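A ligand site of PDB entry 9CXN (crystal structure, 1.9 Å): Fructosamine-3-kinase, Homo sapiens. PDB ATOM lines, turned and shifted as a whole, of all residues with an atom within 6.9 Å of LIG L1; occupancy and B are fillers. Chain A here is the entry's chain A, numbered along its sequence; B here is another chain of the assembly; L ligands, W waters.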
ATOM      1  N   CYS A 133       1.908  25.669  22.971  1.00  0.00           N
ATOM      2  CA  CYS A 133       1.660  24.222  23.009  1.00  0.00           C
ATOM      3  C   CYS A 133       1.865  23.820  24.460  1.00  0.00           C
ATOM      4  O   CYS A 133       2.998  23.583  24.887  1.00  0.00           O
ATOM      5  CB  CYS A 133       2.580  23.438  22.048  1.00  0.00           C
ATOM      6  SG  CYS A 133       2.077  21.673  21.693  1.00  0.00           S
ATOM      7  N   GLY A 134       0.777  23.731  25.214  1.00  0.00           N
ATOM      8  CA  GLY A 134       0.887  23.656  26.674  1.00  0.00           C
ATOM      9  C   GLY A 134       1.135  25.043  27.257  1.00  0.00           C
ATOM     10  O   GLY A 134       0.383  25.963  26.974  1.00  0.00           O
ATOM     11  N   PHE A 135       2.176  25.205  28.047  1.00  0.00           N
ATOM     12  CA  PHE A 135       2.459  26.465  28.722  1.00  0.00           C
ATOM     13  C   PHE A 135       3.531  27.340  28.052  1.00  0.00           C
ATOM     14  O   PHE A 135       3.528  28.557  28.258  1.00  0.00           O
ATOM     15  CB  PHE A 135       2.812  26.126  30.202  1.00  0.00           C
ATOM     16  CG  PHE A 135       3.292  27.258  31.047  1.00  0.00           C
ATOM     17  CD1 PHE A 135       4.630  27.655  31.052  1.00  0.00           C
ATOM     18  CD2 PHE A 135       2.390  27.931  31.901  1.00  0.00           C
ATOM     19  CE1 PHE A 135       5.076  28.717  31.892  1.00  0.00           C
ATOM     20  CE2 PHE A 135       2.828  29.002  32.737  1.00  0.00           C
ATOM     21  CZ  PHE A 135       4.168  29.391  32.719  1.00  0.00           C
ATOM     22  N   ILE A 136       4.377  26.807  27.177  1.00  0.00           N
ATOM     23  CA  ILE A 136       5.513  27.554  26.628  1.00  0.00           C
ATOM     24  C   ILE A 136       5.095  28.304  25.376  1.00  0.00           C
ATOM     25  O   ILE A 136       4.649  27.674  24.414  1.00  0.00           O
ATOM     26  CB  ILE A 136       6.707  26.645  26.337  1.00  0.00           C
ATOM     27  CG1 ILE A 136       6.949  25.626  27.487  1.00  0.00           C
ATOM     28  CG2 ILE A 136       7.873  27.446  25.742  1.00  0.00           C
ATOM     29  CD1 ILE A 136       8.243  24.822  27.304  1.00  0.00           C
ATOM     30  N   GLY A 198      -2.703  21.774  16.196  1.00  0.00           N
ATOM     31  CA  GLY A 198      -1.386  22.013  16.776  1.00  0.00           C
ATOM     32  C   GLY A 198      -1.052  21.200  18.029  1.00  0.00           C
ATOM     33  O   GLY A 198       0.113  21.156  18.448  1.00  0.00           O
ATOM     34  N   ASP A 199      -2.043  20.565  18.633  1.00  0.00           N
ATOM     35  CA  ASP A 199      -1.825  19.800  19.865  1.00  0.00           C
ATOM     36  C   ASP A 199      -2.827  18.654  19.947  1.00  0.00           C
ATOM     37  O   ASP A 199      -3.581  18.497  20.938  1.00  0.00           O
ATOM     38  CB  ASP A 199      -1.955  20.731  21.076  1.00  0.00           C
ATOM     39  CG  ASP A 199      -1.337  20.074  22.370  1.00  0.00           C
ATOM     40  OD1 ASP A 199      -0.549  19.132  22.199  1.00  0.00           O
ATOM     41  OD2 ASP A 199      -1.634  20.505  23.496  1.00  0.00           O
ATOM     42  N   LEU A 200      -2.895  17.855  18.885  1.00  0.00           N
ATOM     43  CA  LEU A 200      -4.025  16.924  18.743  1.00  0.00           C
ATOM     44  C   LEU A 200      -3.734  15.593  19.429  1.00  0.00           C
ATOM     45  O   LEU A 200      -3.710  14.518  18.835  1.00  0.00           O
ATOM     46  CB  LEU A 200      -4.325  16.704  17.239  1.00  0.00           C
ATOM     47  CG  LEU A 200      -5.759  16.167  17.064  1.00  0.00           C
ATOM     48  CD1 LEU A 200      -6.778  17.324  17.100  1.00  0.00           C
ATOM     49  CD2 LEU A 200      -5.889  15.296  15.743  1.00  0.00           C
ATOM     50  N   TRP A 201      -3.367  15.652  20.709  1.00  0.00           N
ATOM     51  CA  TRP A 201      -3.289  14.350  21.323  1.00  0.00           C
ATOM     52  C   TRP A 201      -4.667  13.873  21.795  1.00  0.00           C
ATOM     53  O   TRP A 201      -5.658  14.604  21.757  1.00  0.00           O
ATOM     54  CB  TRP A 201      -2.278  14.366  22.423  1.00  0.00           C
ATOM     55  CG  TRP A 201      -2.776  14.977  23.703  1.00  0.00           C
ATOM     56  CD1 TRP A 201      -3.130  16.305  23.889  1.00  0.00           C
ATOM     57  CD2 TRP A 201      -2.954  14.323  25.005  1.00  0.00           C
ATOM     58  NE1 TRP A 201      -3.508  16.503  25.249  1.00  0.00           N
ATOM     59  CE2 TRP A 201      -3.442  15.317  25.904  1.00  0.00           C
ATOM     60  CE3 TRP A 201      -2.819  13.006  25.452  1.00  0.00           C
ATOM     61  CZ2 TRP A 201      -3.756  15.032  27.301  1.00  0.00           C
ATOM     62  CZ3 TRP A 201      -3.143  12.724  26.808  1.00  0.00           C
ATOM     63  CH2 TRP A 201      -3.570  13.739  27.724  1.00  0.00           C
ATOM     64  N   ASN A 204      -7.081  15.846  23.908  1.00  0.00           N
ATOM     65  CA  ASN A 204      -7.702  17.080  23.407  1.00  0.00           C
ATOM     66  C   ASN A 204      -8.790  16.866  22.369  1.00  0.00           C
ATOM     67  O   ASN A 204      -9.173  17.813  21.668  1.00  0.00           O
ATOM     68  CB  ASN A 204      -6.613  18.008  22.824  1.00  0.00           C
ATOM     69  CG  ASN A 204      -5.766  18.683  23.900  1.00  0.00           C
ATOM     70  OD1 ASN A 204      -6.199  18.772  25.083  1.00  0.00           O
ATOM     71  ND2 ASN A 204      -4.568  19.074  23.543  1.00  0.00           N
ATOM     72  N   ASP A 216      -8.518  22.824  23.165  1.00  0.00           N
ATOM     73  CA  ASP A 216      -7.172  23.136  23.605  1.00  0.00           C
ATOM     74  C   ASP A 216      -6.192  23.276  22.422  1.00  0.00           C
ATOM     75  O   ASP A 216      -5.080  22.776  22.500  1.00  0.00           O
ATOM     76  CB  ASP A 216      -6.674  22.015  24.514  1.00  0.00           C
ATOM     77  CG  ASP A 216      -5.594  22.466  25.477  1.00  0.00           C
ATOM     78  OD1 ASP A 216      -5.360  23.703  25.550  1.00  0.00           O
ATOM     79  OD2 ASP A 216      -4.935  21.575  26.096  1.00  0.00           O
ATOM     80  N   ILE A 230       1.753  13.740  17.388  1.00  0.00           N
ATOM     81  CA  ILE A 230       1.409  13.594  18.780  1.00  0.00           C
ATOM     82  C   ILE A 230       0.230  12.619  18.923  1.00  0.00           C
ATOM     83  O   ILE A 230       0.174  11.893  19.915  1.00  0.00           O
ATOM     84  CB  ILE A 230       1.101  14.976  19.440  1.00  0.00           C
ATOM     85  CG1 ILE A 230       1.065  14.829  20.980  1.00  0.00           C
ATOM     86  CG2 ILE A 230      -0.258  15.570  18.968  1.00  0.00           C
ATOM     87  CD1 ILE A 230       1.029  16.238  21.790  1.00  0.00           C
ATOM     88  N   PHE A 234       1.275   9.144  21.475  1.00  0.00           N
ATOM     89  CA  PHE A 234       0.713   8.817  22.795  1.00  0.00           C
ATOM     90  C   PHE A 234      -0.540   7.938  22.700  1.00  0.00           C
ATOM     91  O   PHE A 234      -1.198   7.683  23.706  1.00  0.00           O
ATOM     92  CB  PHE A 234       0.413  10.122  23.535  1.00  0.00           C
ATOM     93  CG  PHE A 234       1.641  10.931  23.857  1.00  0.00           C
ATOM     94  CD1 PHE A 234       2.650  10.398  24.662  1.00  0.00           C
ATOM     95  CD2 PHE A 234       1.775  12.229  23.376  1.00  0.00           C
ATOM     96  CE1 PHE A 234       3.793  11.147  24.948  1.00  0.00           C
ATOM     97  CE2 PHE A 234       2.868  13.013  23.705  1.00  0.00           C
ATOM     98  CZ  PHE A 234       3.897  12.482  24.498  1.00  0.00           C
ATOM     99  N   ASN A 266       7.758  16.876  19.885  1.00  0.00           N
ATOM    100  CA  ASN A 266       6.847  16.702  21.014  1.00  0.00           C
ATOM    101  C   ASN A 266       7.577  16.156  22.246  1.00  0.00           C
ATOM    102  O   ASN A 266       7.335  16.596  23.396  1.00  0.00           O
ATOM    103  CB  ASN A 266       5.674  15.800  20.622  1.00  0.00           C
ATOM    104  CG  ASN A 266       4.670  16.570  19.738  1.00  0.00           C
ATOM    105  OD1 ASN A 266       4.009  17.451  20.232  1.00  0.00           O
ATOM    106  ND2 ASN A 266       4.665  16.287  18.402  1.00  0.00           N
ATOM    107  N   ASN A 269       9.429  19.107  23.774  1.00  0.00           N
ATOM    108  CA  ASN A 269       8.430  19.918  24.486  1.00  0.00           C
ATOM    109  C   ASN A 269       8.033  19.274  25.818  1.00  0.00           C
ATOM    110  O   ASN A 269       7.814  19.966  26.843  1.00  0.00           O
ATOM    111  CB  ASN A 269       7.188  20.068  23.590  1.00  0.00           C
ATOM    112  CG  ASN A 269       6.212  21.114  24.140  1.00  0.00           C
ATOM    113  OD1 ASN A 269       6.621  22.201  24.532  1.00  0.00           O
ATOM    114  ND2 ASN A 269       4.910  20.790  24.118  1.00  0.00           N
ATOM    115  N   HIS A 270       7.957  17.954  25.848  1.00  0.00           N
ATOM    116  CA  HIS A 270       7.615  17.249  27.090  1.00  0.00           C
ATOM    117  C   HIS A 270       8.755  17.296  28.096  1.00  0.00           C
ATOM    118  O   HIS A 270       8.521  17.431  29.303  1.00  0.00           O
ATOM    119  CB  HIS A 270       7.195  15.791  26.818  1.00  0.00           C
ATOM    120  CG  HIS A 270       5.731  15.657  26.476  1.00  0.00           C
ATOM    121  ND1 HIS A 270       5.170  16.221  25.352  1.00  0.00           N
ATOM    122  CD2 HIS A 270       4.691  15.133  27.180  1.00  0.00           C
ATOM    123  CE1 HIS A 270       3.861  16.035  25.364  1.00  0.00           C
ATOM    124  NE2 HIS A 270       3.545  15.372  26.472  1.00  0.00           N
ATOM    125  N   HIS A 273       8.539  20.693  29.567  1.00  0.00           N
ATOM    126  CA  HIS A 273       7.394  20.821  30.473  1.00  0.00           C
ATOM    127  C   HIS A 273       7.541  20.008  31.762  1.00  0.00           C
ATOM    128  O   HIS A 273       7.174  20.489  32.849  1.00  0.00           O
ATOM    129  CB  HIS A 273       6.102  20.431  29.775  1.00  0.00           C
ATOM    130  CG  HIS A 273       5.489  21.538  28.993  1.00  0.00           C
ATOM    131  ND1 HIS A 273       5.912  21.878  27.706  1.00  0.00           N
ATOM    132  CD2 HIS A 273       4.567  22.472  29.340  1.00  0.00           C
ATOM    133  CE1 HIS A 273       5.203  22.912  27.283  1.00  0.00           C
ATOM    134  NE2 HIS A 273       4.408  23.317  28.260  1.00  0.00           N
ATOM    135  N   PHE A 274       8.019  18.788  31.664  1.00  0.00           N
ATOM    136  CA  PHE A 274       7.902  17.775  32.708  1.00  0.00           C
ATOM    137  C   PHE A 274       9.245  17.204  33.149  1.00  0.00           C
ATOM    138  O   PHE A 274       9.266  16.312  33.996  1.00  0.00           O
ATOM    139  CB  PHE A 274       6.979  16.639  32.212  1.00  0.00           C
ATOM    140  CG  PHE A 274       5.680  17.131  31.660  1.00  0.00           C
ATOM    141  CD1 PHE A 274       4.760  17.817  32.468  1.00  0.00           C
ATOM    142  CD2 PHE A 274       5.314  16.875  30.336  1.00  0.00           C
ATOM    143  CE1 PHE A 274       3.566  18.299  31.956  1.00  0.00           C
ATOM    144  CE2 PHE A 274       4.110  17.326  29.839  1.00  0.00           C
ATOM    145  CZ  PHE A 274       3.226  18.023  30.647  1.00  0.00           C
ATOM    146  N   TYR A 278      11.632  12.749  30.053  1.00  0.00           N
ATOM    147  CA  TYR A 278      11.566  12.766  28.578  1.00  0.00           C
ATOM    148  C   TYR A 278      12.918  12.959  27.895  1.00  0.00           C
ATOM    149  O   TYR A 278      12.980  13.121  26.670  1.00  0.00           O
ATOM    150  CB  TYR A 278      10.583  13.822  28.140  1.00  0.00           C
ATOM    151  CG  TYR A 278       9.207  13.416  28.479  1.00  0.00           C
ATOM    152  CD1 TYR A 278       8.507  12.535  27.651  1.00  0.00           C
ATOM    153  CD2 TYR A 278       8.569  13.923  29.623  1.00  0.00           C
ATOM    154  CE1 TYR A 278       7.190  12.166  27.935  1.00  0.00           C
ATOM    155  CE2 TYR A 278       7.261  13.531  29.947  1.00  0.00           C
ATOM    156  CZ  TYR A 278       6.577  12.673  29.096  1.00  0.00           C
ATOM    157  OH  TYR A 278       5.285  12.327  29.339  1.00  0.00           O
ATOM    158  N   PHE B 274       2.494  18.236  37.335  1.00  0.00           N
ATOM    159  CA  PHE B 274       1.945  18.933  36.196  1.00  0.00           C
ATOM    160  C   PHE B 274       2.947  19.816  35.506  1.00  0.00           C
ATOM    161  O   PHE B 274       2.587  20.467  34.516  1.00  0.00           O
ATOM    162  CB  PHE B 274       0.730  19.783  36.575  1.00  0.00           C
ATOM    163  CG  PHE B 274      -0.345  19.006  37.290  1.00  0.00           C
ATOM    164  CD1 PHE B 274      -0.932  17.878  36.709  1.00  0.00           C
ATOM    165  CD2 PHE B 274      -0.778  19.388  38.574  1.00  0.00           C
ATOM    166  CE1 PHE B 274      -1.900  17.117  37.386  1.00  0.00           C
ATOM    167  CE2 PHE B 274      -1.788  18.635  39.261  1.00  0.00           C
ATOM    168  CZ  PHE B 274      -2.347  17.509  38.674  1.00  0.00           C
HETATM  169  N1  LIG L   1       0.893  15.086  27.135  1.00  0.00           N
HETATM  170  C1  LIG L   1       0.058  16.088  26.310  1.00  0.00           C
HETATM  171  C2  LIG L   1      -0.136  17.558  26.790  1.00  0.00           C
HETATM  172  O1  LIG L   1      -0.249  17.867  27.996  1.00  0.00           O
HETATM  173  C3  LIG L   1       0.601  15.087  28.599  1.00  0.00           C
HETATM  174  C4  LIG L   1       1.465  14.020  29.377  1.00  0.00           C
HETATM  175  C5  LIG L   1       1.414  12.653  27.390  1.00  0.00           C
HETATM  176  C6  LIG L   1       0.600  13.730  26.645  1.00  0.00           C
HETATM  177  C7  LIG L   1      -0.311  18.711  25.744  1.00  0.00           C
HETATM  178  C8  LIG L   1       1.058  19.179  25.135  1.00  0.00           C
HETATM  179  C9  LIG L   1       2.222  19.427  26.165  1.00  0.00           C
HETATM  180  C10 LIG L   1       2.106  20.586  27.172  1.00  0.00           C
HETATM  181  O2  LIG L   1       1.108  12.669  28.800  1.00  0.00           O
HETATM  182  O3  LIG L   1       0.937  20.490  27.980  1.00  0.00           O
HETATM  183  O4  LIG L   1       2.246  18.237  26.982  1.00  0.00           O
HETATM  184  O5  LIG L   1       1.409  18.358  24.026  1.00  0.00           O
HETATM  185  O6  LIG L   1      -1.154  19.788  26.214  1.00  0.00           O
HETATM  186  P1  LG2 L   2      -3.480  21.700  31.102  1.00  0.00           P
HETATM  187  O1  LG2 L   2      -3.499  23.037  31.809  1.00  0.00           O
HETATM  188  O2  LG2 L   2      -2.339  21.748  29.999  1.00  0.00           O
HETATM  189  O3  LG2 L   2      -3.141  20.570  32.171  1.00  0.00           O
HETATM  190  P2  LG2 L   2      -5.916  22.608  29.759  1.00  0.00           P
HETATM  191  O4  LG2 L   2      -5.928  23.775  30.713  1.00  0.00           O
HETATM  192  O5  LG2 L   2      -5.164  23.168  28.499  1.00  0.00           O
HETATM  193  N1  LG2 L   2      -5.009  21.324  30.387  1.00  0.00           N
HETATM  194  P3  LG2 L   2      -8.084  21.469  28.160  1.00  0.00           P
HETATM  195  O6  LG2 L   2      -7.184  20.434  27.564  1.00  0.00           O
HETATM  196  O7  LG2 L   2      -8.510  22.504  27.098  1.00  0.00           O
HETATM  197  O8  LG2 L   2      -7.413  22.179  29.462  1.00  0.00           O
HETATM  198  O9  LG2 L   2      -9.340  20.742  28.789  1.00  0.00           O
HETATM  199  C1  LG2 L   2      -9.088  19.752  29.830  1.00  0.00           C
HETATM  200  C2  LG2 L   2     -10.324  18.976  30.218  1.00  0.00           C
HETATM  201  O10 LG2 L   2     -11.388  19.896  30.545  1.00  0.00           O
HETATM  202  C3  LG2 L   2     -10.894  18.061  29.125  1.00  0.00           C
HETATM  203  O11 LG2 L   2     -10.269  16.786  29.150  1.00  0.00           O
HETATM  204  C4  LG2 L   2     -12.395  18.043  29.448  1.00  0.00           C
HETATM  205  O12 LG2 L   2     -12.801  17.068  30.409  1.00  0.00           O
HETATM  206  C5  LG2 L   2     -12.608  19.457  29.994  1.00  0.00           C
HETATM  207  N2  LG2 L   2     -13.075  20.436  28.995  1.00  0.00           N
HETATM  208  C6  LG2 L   2     -12.305  21.157  28.107  1.00  0.00           C
HETATM  209  N3  LG2 L   2     -13.007  21.968  27.346  1.00  0.00           N
HETATM  210  C7  LG2 L   2     -14.313  21.759  27.748  1.00  0.00           C
HETATM  211  C8  LG2 L   2     -15.546  22.322  27.339  1.00  0.00           C
HETATM  212  N4  LG2 L   2     -15.655  23.241  26.369  1.00  0.00           N
HETATM  213  N5  LG2 L   2     -16.675  21.902  27.961  1.00  0.00           N
HETATM  214  C9  LG2 L   2     -16.567  20.983  28.931  1.00  0.00           C
HETATM  215  N6  LG2 L   2     -15.470  20.400  29.406  1.00  0.00           N
HETATM  216  C10 LG2 L   2     -14.371  20.820  28.777  1.00  0.00           C
HETATM  217  O   HOH W   1       4.071  18.191  22.884  1.00  0.00           O
HETATM  218  O   HOH W   2      -3.956  19.350  27.206  1.00  0.00           O
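Water W1 lies within hydrogen-bond range of the side-chain amide oxygen (OD1) of Asn 266 (2.8 Å), an oxygen (O5) of LIG L1 (2.9 Å), the side-chain amide nitrogen (ND2) of Asn 269 (3.0 Å) and a ring nitrogen (ND1) of His 270 (3.3 Å). Water W2 lies within hydrogen-bond range of the side-chain carboxylate (OD2) of Asp 216, an oxygen (O6) of LIG L1, the side-chain amide oxygen (OD1) of Asn 204, an oxygen (O6) of LG2 L2 and the indole nitrogen (NE1) of Trp 201.
O of Asn 266 is in hydrogen-bond range of ND1 of His 270 (2.9 Å). The side-chain carboxylate (OD1) of Asp 199 sits at hydrogen-bond distance from the side-chain sulfur (SG) of Cys 133, 3.7 Å away. ND2 of Asn 204 sits at hydrogen-bond distance from O of Asp 199. The indole nitrogen (NE1) of Trp 201 sits close to the side-chain amide nitrogen (ND2) of Asn 204 (3.3 Å). A ring nitrogen (ND1) of His 273 lies within hydrogen-bond range of the backbone carbonyl oxygen of Asn 269 (2.8 Å). The side-chain amide nitrogen (ND2) of Asn 269 lies within hydrogen-bond range of the backbone carbonyl oxygen (O) of Cys 133 (3.5 Å). A ring nitrogen (NE2) of His 273 sits at hydrogen-bond distance from the backbone NH (N) of Phe 135 (2.9 Å).
O of Cys 133 touches C10 of LIG L1, at 3.9 Å. Gly 134 touches LIG L1. Trp 201 touches LIG L1 (CE2 to C1, 3.6 Å). CD1 of Ile 230 touches O5 of LIG L1, 3.1 Å away. Phe 234 touches LIG L1. ND2 of Asn 269 touches C9 of LIG L1 (3.6 Å). His 273 touches LIG L1. CE2 of Phe 274 of chain A touches O4 of LIG L1 (3.5 Å). Hydrophobic or aromatic side chains that line LIG L1: Trp 201, Ile 230, Phe 234, His 270, His 273 and Phe 274 of chain A. The nearest printed residue that does not touch LIG L1 is Tyr 278 (4.2 Å).
A ring nitrogen (NE2) of His 270 sits close to an oxygen (O4) of LIG L1 (3.2 Å). An oxygen (O5) of LIG L1 is in hydrogen-bond range of the side-chain carboxylate of Asp 199 (2.8 Å). The side-chain carboxylate of Asp 216 lies close to an oxygen (O5) of LG2 L2, 2.9 Å away. OD1 of Asn 204 sits close to O6 of LG2 L2 (3.1 Å).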
